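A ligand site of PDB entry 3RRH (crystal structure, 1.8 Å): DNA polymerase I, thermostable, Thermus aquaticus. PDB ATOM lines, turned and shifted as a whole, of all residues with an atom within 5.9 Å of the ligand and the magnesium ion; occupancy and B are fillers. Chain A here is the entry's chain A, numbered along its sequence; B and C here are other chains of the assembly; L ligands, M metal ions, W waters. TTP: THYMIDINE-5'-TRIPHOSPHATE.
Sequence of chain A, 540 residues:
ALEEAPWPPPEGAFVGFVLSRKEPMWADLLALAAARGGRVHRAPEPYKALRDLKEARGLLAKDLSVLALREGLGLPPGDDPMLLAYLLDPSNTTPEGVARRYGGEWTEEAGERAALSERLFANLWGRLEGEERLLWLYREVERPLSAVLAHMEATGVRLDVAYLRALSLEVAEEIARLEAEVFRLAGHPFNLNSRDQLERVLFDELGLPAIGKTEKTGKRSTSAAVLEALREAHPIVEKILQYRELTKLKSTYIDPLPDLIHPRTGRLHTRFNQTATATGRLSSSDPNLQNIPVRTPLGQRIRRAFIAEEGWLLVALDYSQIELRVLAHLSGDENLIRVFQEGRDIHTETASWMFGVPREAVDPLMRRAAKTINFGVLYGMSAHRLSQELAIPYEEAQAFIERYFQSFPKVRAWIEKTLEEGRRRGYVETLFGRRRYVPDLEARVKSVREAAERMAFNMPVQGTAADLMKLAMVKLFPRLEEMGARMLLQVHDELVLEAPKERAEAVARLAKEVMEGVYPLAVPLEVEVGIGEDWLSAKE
The side-chain hydroxyl (OH) of Tyr 379 lies within hydrogen-bond range of a nitrogen (N3) of the ligand (2.8 Å). The side-chain amide nitrogen (NE2) of Gln 321 is in hydrogen-bond range of an oxygen (O2B) of the ligand. A ring nitrogen (NE2) of His 347 is in hydrogen-bond range of an oxygen (O2B) of the ligand, 2.8 Å away. The side-chain amino group (NZ) of Lys 371 is in salt-bridge range of an oxygen (O1A) of the ligand (2.7 Å). NH2 of Arg 367 lies within salt-bridge range of O3G of the ligand (2.8 Å).
O2 of 2DT 12 of chain B sits at hydrogen-bond distance from the guanidinium group (NH1) of Arg 281 (2.8 Å). The guanidinium group (NH1) of Arg 295 is in salt-bridge range of OP2 of 2DT 12 of chain B. OD2 of Asp 345 lies within salt-bridge range of NH2 of Arg 367 (3.0 Å). The backbone carbonyl oxygen (O) of Asp 493 is in hydrogen-bond range of the backbone NH (N) of Tyr 319 (2.9 Å). N3 of 2DT 12 of chain B sits close to N1 of DA 5 of chain C (2.7 Å). N of His 347 is in hydrogen-bond range of OD1 of Asp 345, at 2.9 Å.
N3 of 2DT 12 of chain B lies close to an oxygen (O2) of the ligand (3.4 Å). Phe 375 touches the ligand (CB to O4, 3.4 Å). OD2 of Asp 493 touches C3' of the ligand (3.6 Å). Hydrophobic or aromatic side chains within 4 Å of the ligand: His 347, Phe 375 and Tyr 379. Within 4 Å of the ligand: Gln 321, His 347, Arg 367, Lys 371, Phe 375, Tyr 379, Asp 493 and 2DT 12 of chain B. The nearest printed residue that does not touch the ligand is Arg 295 (4.2 Å).
No residue comes within 4 Å of the magnesium ion. The nearest printed residue that does not touch the magnesium ion is Glu 528 (4.9 Å).
The magnesium ion is bound by O2A of the ligand (1.9 Å), O1G of the ligand (2.1 Å), O1B of the ligand (2.1 Å), water W7 (2.1 Å) and water W1 (2.1 Å). The magnesium ion has five donor atoms within binding distance.
Water W2 lies within hydrogen-bond range of O2 of the ligand and OE1 of Glu 323. Water W4 bridges N of Gln 321 and O2B of the ligand. Water W6 lies within hydrogen-bond range of the side-chain hydroxyl of Tyr 379 (2.5 Å), the side-chain carboxylate of Glu 323 (2.8 Å) and an oxygen (O2) of the ligand (3.1 Å).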
ATOM      1  N   ARG A 281     -21.029 -16.503  27.651  1.00  0.00           N
ATOM      2  CA  ARG A 281     -20.066 -15.437  27.376  1.00  0.00           C
ATOM      3  C   ARG A 281     -18.778 -15.688  28.135  1.00  0.00           C
ATOM      4  O   ARG A 281     -18.777 -16.368  29.172  1.00  0.00           O
ATOM      5  CB  ARG A 281     -20.629 -14.081  27.792  1.00  0.00           C
ATOM      6  CG  ARG A 281     -21.533 -13.416  26.762  1.00  0.00           C
ATOM      7  CD  ARG A 281     -21.728 -11.961  27.170  1.00  0.00           C
ATOM      8  NE  ARG A 281     -22.462 -11.186  26.165  1.00  0.00           N
ATOM      9  CZ  ARG A 281     -22.756  -9.903  26.298  1.00  0.00           C
ATOM     10  NH1 ARG A 281     -22.386  -9.256  27.399  1.00  0.00           N
ATOM     11  NH2 ARG A 281     -23.431  -9.269  25.347  1.00  0.00           N
ATOM     12  N   ARG A 295     -17.347   5.800  25.548  1.00  0.00           N
ATOM     13  CA  ARG A 295     -18.438   6.700  25.202  1.00  0.00           C
ATOM     14  C   ARG A 295     -18.125   8.184  25.394  1.00  0.00           C
ATOM     15  O   ARG A 295     -18.305   8.984  24.474  1.00  0.00           O
ATOM     16  CB  ARG A 295     -19.723   6.317  25.938  1.00  0.00           C
ATOM     17  CG  ARG A 295     -20.336   5.043  25.401  1.00  0.00           C
ATOM     18  CD  ARG A 295     -21.715   4.793  25.980  1.00  0.00           C
ATOM     19  NE  ARG A 295     -22.410   3.757  25.221  1.00  0.00           N
ATOM     20  CZ  ARG A 295     -22.046   2.482  25.178  1.00  0.00           C
ATOM     21  NH1 ARG A 295     -20.988   2.066  25.879  1.00  0.00           N
ATOM     22  NH2 ARG A 295     -22.737   1.620  24.464  1.00  0.00           N
ATOM     23  N   TYR A 319     -18.811  -7.228  15.314  1.00  0.00           N
ATOM     24  CA  TYR A 319     -20.031  -7.662  14.674  1.00  0.00           C
ATOM     25  C   TYR A 319     -21.070  -6.560  14.835  1.00  0.00           C
ATOM     26  O   TYR A 319     -21.214  -6.006  15.925  1.00  0.00           O
ATOM     27  CB  TYR A 319     -20.588  -8.932  15.333  1.00  0.00           C
ATOM     28  CG  TYR A 319     -19.891 -10.215  14.945  1.00  0.00           C
ATOM     29  CD1 TYR A 319     -20.090 -10.797  13.702  1.00  0.00           C
ATOM     30  CD2 TYR A 319     -19.080 -10.881  15.865  1.00  0.00           C
ATOM     31  CE1 TYR A 319     -19.472 -11.998  13.364  1.00  0.00           C
ATOM     32  CE2 TYR A 319     -18.459 -12.077  15.541  1.00  0.00           C
ATOM     33  CZ  TYR A 319     -18.653 -12.622  14.285  1.00  0.00           C
ATOM     34  OH  TYR A 319     -18.030 -13.814  13.974  1.00  0.00           O
ATOM     35  N   SER A 320     -21.760  -6.245  13.751  1.00  0.00           N
ATOM     36  CA  SER A 320     -22.853  -5.284  13.814  1.00  0.00           C
ATOM     37  C   SER A 320     -24.151  -5.933  14.288  1.00  0.00           C
ATOM     38  O   SER A 320     -24.647  -6.858  13.669  1.00  0.00           O
ATOM     39  CB  SER A 320     -23.078  -4.664  12.424  1.00  0.00           C
ATOM     40  OG  SER A 320     -21.880  -4.076  11.942  1.00  0.00           O
ATOM     41  N   GLN A 321     -24.688  -5.427  15.398  1.00  0.00           N
ATOM     42  CA  GLN A 321     -25.960  -5.899  15.972  1.00  0.00           C
ATOM     43  C   GLN A 321     -26.075  -7.415  15.970  1.00  0.00           C
ATOM     44  O   GLN A 321     -27.100  -7.956  15.551  1.00  0.00           O
ATOM     45  CB  GLN A 321     -27.161  -5.321  15.211  1.00  0.00           C
ATOM     46  CG  GLN A 321     -27.193  -3.805  15.142  1.00  0.00           C
ATOM     47  CD  GLN A 321     -26.476  -3.267  13.924  1.00  0.00           C
ATOM     48  OE1 GLN A 321     -26.430  -3.908  12.879  1.00  0.00           O
ATOM     49  NE2 GLN A 321     -25.909  -2.078  14.053  1.00  0.00           N
ATOM     50  N   GLU A 323     -26.627  -9.636  18.295  1.00  0.00           N
ATOM     51  CA  GLU A 323     -27.728 -10.217  19.072  1.00  0.00           C
ATOM     52  C   GLU A 323     -29.074 -10.034  18.367  1.00  0.00           C
ATOM     53  O   GLU A 323     -29.935 -10.917  18.410  1.00  0.00           O
ATOM     54  CB  GLU A 323     -27.748  -9.686  20.506  1.00  0.00           C
ATOM     55  CG  GLU A 323     -26.575 -10.220  21.320  1.00  0.00           C
ATOM     56  CD  GLU A 323     -26.590  -9.790  22.775  1.00  0.00           C
ATOM     57  OE1 GLU A 323     -27.454  -8.973  23.155  1.00  0.00           O
ATOM     58  OE2 GLU A 323     -25.723 -10.259  23.543  1.00  0.00           O
ATOM     59  N   ASP A 345     -29.547  -0.081   7.241  1.00  0.00           N
ATOM     60  CA  ASP A 345     -29.257   0.319   8.619  1.00  0.00           C
ATOM     61  C   ASP A 345     -30.394  -0.125   9.534  1.00  0.00           C
ATOM     62  O   ASP A 345     -31.522   0.363   9.439  1.00  0.00           O
ATOM     63  CB  ASP A 345     -29.030   1.829   8.722  1.00  0.00           C
ATOM     64  CG  ASP A 345     -28.789   2.283  10.145  1.00  0.00           C
ATOM     65  OD1 ASP A 345     -29.590   1.930  11.046  1.00  0.00           O
ATOM     66  OD2 ASP A 345     -27.793   3.012  10.378  1.00  0.00           O
ATOM     67  N   HIS A 347     -31.281   0.223  12.737  1.00  0.00           N
ATOM     68  CA  HIS A 347     -31.991   1.137  13.614  1.00  0.00           C
ATOM     69  C   HIS A 347     -32.838   2.151  12.828  1.00  0.00           C
ATOM     70  O   HIS A 347     -33.966   2.453  13.201  1.00  0.00           O
ATOM     71  CB  HIS A 347     -31.006   1.836  14.555  1.00  0.00           C
ATOM     72  CG  HIS A 347     -30.161   0.885  15.338  1.00  0.00           C
ATOM     73  ND1 HIS A 347     -30.685  -0.155  16.064  1.00  0.00           N
ATOM     74  CD2 HIS A 347     -28.815   0.824  15.511  1.00  0.00           C
ATOM     75  CE1 HIS A 347     -29.708  -0.831  16.648  1.00  0.00           C
ATOM     76  NE2 HIS A 347     -28.563  -0.245  16.326  1.00  0.00           N
ATOM     77  N   ARG A 367     -34.548   7.503  15.275  1.00  0.00           N
ATOM     78  CA  ARG A 367     -33.553   6.433  15.188  1.00  0.00           C
ATOM     79  C   ARG A 367     -33.128   6.008  16.587  1.00  0.00           C
ATOM     80  O   ARG A 367     -32.878   4.840  16.848  1.00  0.00           O
ATOM     81  CB  ARG A 367     -32.332   6.893  14.395  1.00  0.00           C
ATOM     82  CG  ARG A 367     -31.335   5.756  14.140  1.00  0.00           C
ATOM     83  CD  ARG A 367     -30.070   6.250  13.471  1.00  0.00           C
ATOM     84  NE  ARG A 367     -29.235   5.135  13.044  1.00  0.00           N
ATOM     85  CZ  ARG A 367     -28.269   4.598  13.784  1.00  0.00           C
ATOM     86  NH1 ARG A 367     -27.999   5.082  14.991  1.00  0.00           N
ATOM     87  NH2 ARG A 367     -27.573   3.577  13.318  1.00  0.00           N
ATOM     88  N   LYS A 371     -33.371   2.311  18.174  1.00  0.00           N
ATOM     89  CA  LYS A 371     -32.143   1.660  18.630  1.00  0.00           C
ATOM     90  C   LYS A 371     -32.287   1.227  20.085  1.00  0.00           C
ATOM     91  O   LYS A 371     -31.929   0.098  20.449  1.00  0.00           O
ATOM     92  CB  LYS A 371     -30.964   2.611  18.462  1.00  0.00           C
ATOM     93  CG  LYS A 371     -29.642   2.109  19.028  1.00  0.00           C
ATOM     94  CD  LYS A 371     -28.548   3.115  18.731  1.00  0.00           C
ATOM     95  CE  LYS A 371     -27.290   2.831  19.536  1.00  0.00           C
ATOM     96  NZ  LYS A 371     -26.249   3.852  19.260  1.00  0.00           N
ATOM     97  N   PHE A 375     -32.289  -2.894  21.313  1.00  0.00           N
ATOM     98  CA  PHE A 375     -31.519  -3.580  22.344  1.00  0.00           C
ATOM     99  C   PHE A 375     -32.396  -3.919  23.539  1.00  0.00           C
ATOM    100  O   PHE A 375     -32.255  -4.976  24.147  1.00  0.00           O
ATOM    101  CB  PHE A 375     -30.305  -2.755  22.778  1.00  0.00           C
ATOM    102  CG  PHE A 375     -29.216  -2.694  21.747  1.00  0.00           C
ATOM    103  CD1 PHE A 375     -28.382  -3.783  21.560  1.00  0.00           C
ATOM    104  CD2 PHE A 375     -29.055  -1.576  20.952  1.00  0.00           C
ATOM    105  CE1 PHE A 375     -27.388  -3.742  20.613  1.00  0.00           C
ATOM    106  CE2 PHE A 375     -28.054  -1.530  19.995  1.00  0.00           C
ATOM    107  CZ  PHE A 375     -27.226  -2.615  19.816  1.00  0.00           C
ATOM    108  N   GLY A 376     -33.310  -3.019  23.858  1.00  0.00           N
ATOM    109  CA  GLY A 376     -34.189  -3.193  25.004  1.00  0.00           C
ATOM    110  C   GLY A 376     -35.040  -4.438  24.952  1.00  0.00           C
ATOM    111  O   GLY A 376     -35.243  -5.105  25.964  1.00  0.00           O
ATOM    112  N   TYR A 379     -33.739  -7.550  26.504  1.00  0.00           N
ATOM    113  CA  TYR A 379     -33.600  -7.624  27.956  1.00  0.00           C
ATOM    114  C   TYR A 379     -34.952  -7.666  28.662  1.00  0.00           C
ATOM    115  O   TYR A 379     -35.017  -7.877  29.863  1.00  0.00           O
ATOM    116  CB  TYR A 379     -32.841  -6.409  28.483  1.00  0.00           C
ATOM    117  CG  TYR A 379     -31.551  -6.126  27.768  1.00  0.00           C
ATOM    118  CD1 TYR A 379     -30.750  -7.171  27.312  1.00  0.00           C
ATOM    119  CD2 TYR A 379     -31.129  -4.826  27.553  1.00  0.00           C
ATOM    120  CE1 TYR A 379     -29.555  -6.920  26.647  1.00  0.00           C
ATOM    121  CE2 TYR A 379     -29.931  -4.562  26.898  1.00  0.00           C
ATOM    122  CZ  TYR A 379     -29.150  -5.610  26.454  1.00  0.00           C
ATOM    123  OH  TYR A 379     -27.968  -5.347  25.788  1.00  0.00           O
ATOM    124  N   ASP A 493     -18.562  -9.036  21.334  1.00  0.00           N
ATOM    125  CA  ASP A 493     -18.877  -9.056  19.898  1.00  0.00           C
ATOM    126  C   ASP A 493     -17.770  -8.424  19.089  1.00  0.00           C
ATOM    127  O   ASP A 493     -17.938  -8.126  17.913  1.00  0.00           O
ATOM    128  CB  ASP A 493     -20.216  -8.375  19.612  1.00  0.00           C
ATOM    129  CG  ASP A 493     -20.259  -6.923  20.082  1.00  0.00           C
ATOM    130  OD1 ASP A 493     -19.206  -6.353  20.442  1.00  0.00           O
ATOM    131  OD2 ASP A 493     -21.366  -6.347  20.069  1.00  0.00           O
ATOM    132  N   GLU A 528     -17.685  -4.793  11.078  1.00  0.00           N
ATOM    133  CA  GLU A 528     -17.010  -3.520  10.839  1.00  0.00           C
ATOM    134  C   GLU A 528     -15.554  -3.689  11.250  1.00  0.00           C
ATOM    135  O   GLU A 528     -15.275  -4.233  12.314  1.00  0.00           O
ATOM    136  CB  GLU A 528     -17.651  -2.409  11.666  1.00  0.00           C
ATOM    137  CG  GLU A 528     -19.110  -2.139  11.301  1.00  0.00           C
ATOM    138  CD  GLU A 528     -19.719  -1.006  12.115  1.00  0.00           C
ATOM    139  OE1 GLU A 528     -19.257  -0.757  13.252  1.00  0.00           O
ATOM    140  OE2 GLU A 528     -20.662  -0.354  11.606  1.00  0.00           O
ATOM    141  P   2DT B  12     -18.882  -0.955  24.261  1.00  0.00           P
ATOM    142  OP1 2DT B  12     -17.906  -0.774  23.118  1.00  0.00           O
ATOM    143  OP2 2DT B  12     -20.010   0.015  24.493  1.00  0.00           O
ATOM    144  O5' 2DT B  12     -19.503  -2.430  24.206  1.00  0.00           O
ATOM    145  N1  2DT B  12     -22.070  -4.839  26.061  1.00  0.00           N
ATOM    146  C6  2DT B  12     -21.930  -3.504  25.978  1.00  0.00           C
ATOM    147  C2  2DT B  12     -23.112  -5.422  26.791  1.00  0.00           C
ATOM    148  O2  2DT B  12     -23.213  -6.673  26.827  1.00  0.00           O
ATOM    149  N3  2DT B  12     -23.986  -4.656  27.465  1.00  0.00           N
ATOM    150  C4  2DT B  12     -23.896  -3.322  27.451  1.00  0.00           C
ATOM    151  O4  2DT B  12     -24.732  -2.630  28.081  1.00  0.00           O
ATOM    152  C5  2DT B  12     -22.810  -2.676  26.672  1.00  0.00           C
ATOM    153  C5M 2DT B  12     -22.685  -1.173  26.608  1.00  0.00           C
ATOM    154  C2' 2DT B  12     -21.598  -5.850  23.908  1.00  0.00           C
ATOM    155  C5' 2DT B  12     -18.670  -3.537  23.867  1.00  0.00           C
ATOM    156  C4' 2DT B  12     -19.431  -4.862  23.973  1.00  0.00           C
ATOM    157  O4' 2DT B  12     -19.851  -5.118  25.313  1.00  0.00           O
ATOM    158  C1' 2DT B  12     -21.137  -5.722  25.352  1.00  0.00           C
ATOM    159  C3' 2DT B  12     -20.712  -4.868  23.147  1.00  0.00           C
ATOM    160  P    DA C   5     -32.783  -7.409  33.665  1.00  0.00           P
ATOM    161  OP1  DA C   5     -34.063  -8.024  34.058  1.00  0.00           O
ATOM    162  OP2  DA C   5     -31.958  -6.716  34.675  1.00  0.00           O
ATOM    163  O5'  DA C   5     -31.900  -8.542  32.950  1.00  0.00           O
ATOM    164  C5'  DA C   5     -32.525  -9.486  32.083  1.00  0.00           C
ATOM    165  C4'  DA C   5     -31.454 -10.132  31.223  1.00  0.00           C
ATOM    166  O4'  DA C   5     -31.119  -9.213  30.171  1.00  0.00           O
ATOM    167  C3'  DA C   5     -30.139 -10.400  31.945  1.00  0.00           C
ATOM    168  O3'  DA C   5     -30.137 -11.725  32.449  1.00  0.00           O
ATOM    169  C2'  DA C   5     -29.103 -10.269  30.843  1.00  0.00           C
ATOM    170  C1'  DA C   5     -29.728  -9.225  29.932  1.00  0.00           C
ATOM    171  N9   DA C   5     -29.223  -7.856  30.093  1.00  0.00           N
ATOM    172  C8   DA C   5     -29.832  -6.820  30.711  1.00  0.00           C
ATOM    173  N7   DA C   5     -29.148  -5.697  30.666  1.00  0.00           N
ATOM    174  C5   DA C   5     -28.015  -6.051  29.947  1.00  0.00           C
ATOM    175  C6   DA C   5     -26.891  -5.306  29.551  1.00  0.00           C
ATOM    176  N6   DA C   5     -26.740  -4.000  29.834  1.00  0.00           N
ATOM    177  N1   DA C   5     -25.941  -5.957  28.843  1.00  0.00           N
ATOM    178  C2   DA C   5     -26.106  -7.259  28.561  1.00  0.00           C
ATOM    179  N3   DA C   5     -27.117  -8.055  28.891  1.00  0.00           N
ATOM    180  C4   DA C   5     -28.048  -7.369  29.585  1.00  0.00           C
HETATM  181  PA  TTP L   1     -23.675   0.916  19.442  1.00  0.00           P
HETATM  182  O1A TTP L   1     -24.278   2.135  20.101  1.00  0.00           O
HETATM  183  O2A TTP L   1     -22.535   1.306  18.527  1.00  0.00           O
HETATM  184  O3A TTP L   1     -24.803   0.077  18.681  1.00  0.00           O
HETATM  185  PB  TTP L   1     -24.924   0.076  17.076  1.00  0.00           P
HETATM  186  O1B TTP L   1     -23.593  -0.097  16.386  1.00  0.00           O
HETATM  187  O2B TTP L   1     -25.888  -1.009  16.683  1.00  0.00           O
HETATM  188  O3B TTP L   1     -25.561   1.527  16.810  1.00  0.00           O
HETATM  189  PG  TTP L   1     -24.981   2.521  15.682  1.00  0.00           P
HETATM  190  O1G TTP L   1     -23.468   2.507  15.721  1.00  0.00           O
HETATM  191  O2G TTP L   1     -25.473   3.916  15.961  1.00  0.00           O
HETATM  192  O3G TTP L   1     -25.473   2.068  14.335  1.00  0.00           O
HETATM  193  O5' TTP L   1     -23.211  -0.145  20.545  1.00  0.00           O
HETATM  194  C5' TTP L   1     -22.003  -0.881  20.348  1.00  0.00           C
HETATM  195  C4' TTP L   1     -22.182  -2.238  21.023  1.00  0.00           C
HETATM  196  O4' TTP L   1     -22.790  -2.049  22.301  1.00  0.00           O
HETATM  197  C3' TTP L   1     -23.090  -3.148  20.220  1.00  0.00           C
HETATM  198  C2' TTP L   1     -24.049  -3.747  21.232  1.00  0.00           C
HETATM  199  C1' TTP L   1     -23.701  -3.104  22.571  1.00  0.00           C
HETATM  200  N1  TTP L   1     -24.903  -2.588  23.231  1.00  0.00           N
HETATM  201  C2  TTP L   1     -25.583  -3.475  24.090  1.00  0.00           C
HETATM  202  O2  TTP L   1     -25.110  -4.618  24.242  1.00  0.00           O
HETATM  203  N3  TTP L   1     -26.698  -3.096  24.731  1.00  0.00           N
HETATM  204  C4  TTP L   1     -27.193  -1.869  24.565  1.00  0.00           C
HETATM  205  O4  TTP L   1     -28.237  -1.507  25.160  1.00  0.00           O
HETATM  206  C5  TTP L   1     -26.498  -0.915  23.661  1.00  0.00           C
HETATM  207  C5M TTP L   1     -27.032   0.473  23.447  1.00  0.00           C
HETATM  208  C6  TTP L   1     -25.350  -1.343  23.014  1.00  0.00           C
HETATM  209 MG    MG M   1     -22.101   1.308  16.713  1.00  0.00          MG
HETATM  210  O   HOH W   1     -21.082  -0.522  16.693  1.00  0.00           O
HETATM  211  O   HOH W   2     -25.385  -6.866  22.563  1.00  0.00           O
HETATM  212  O   HOH W   3     -20.975  -3.497  17.540  1.00  0.00           O
HETATM  213  O   HOH W   4     -23.550  -3.139  16.710  1.00  0.00           O
HETATM  214  O   HOH W   5     -30.766   0.252  25.077  1.00  0.00           O
HETATM  215  O   HOH W   6     -26.415  -7.243  25.148  1.00  0.00           O
HETATM  216  O   HOH W   7     -21.584   1.305  14.698  1.00  0.00           O
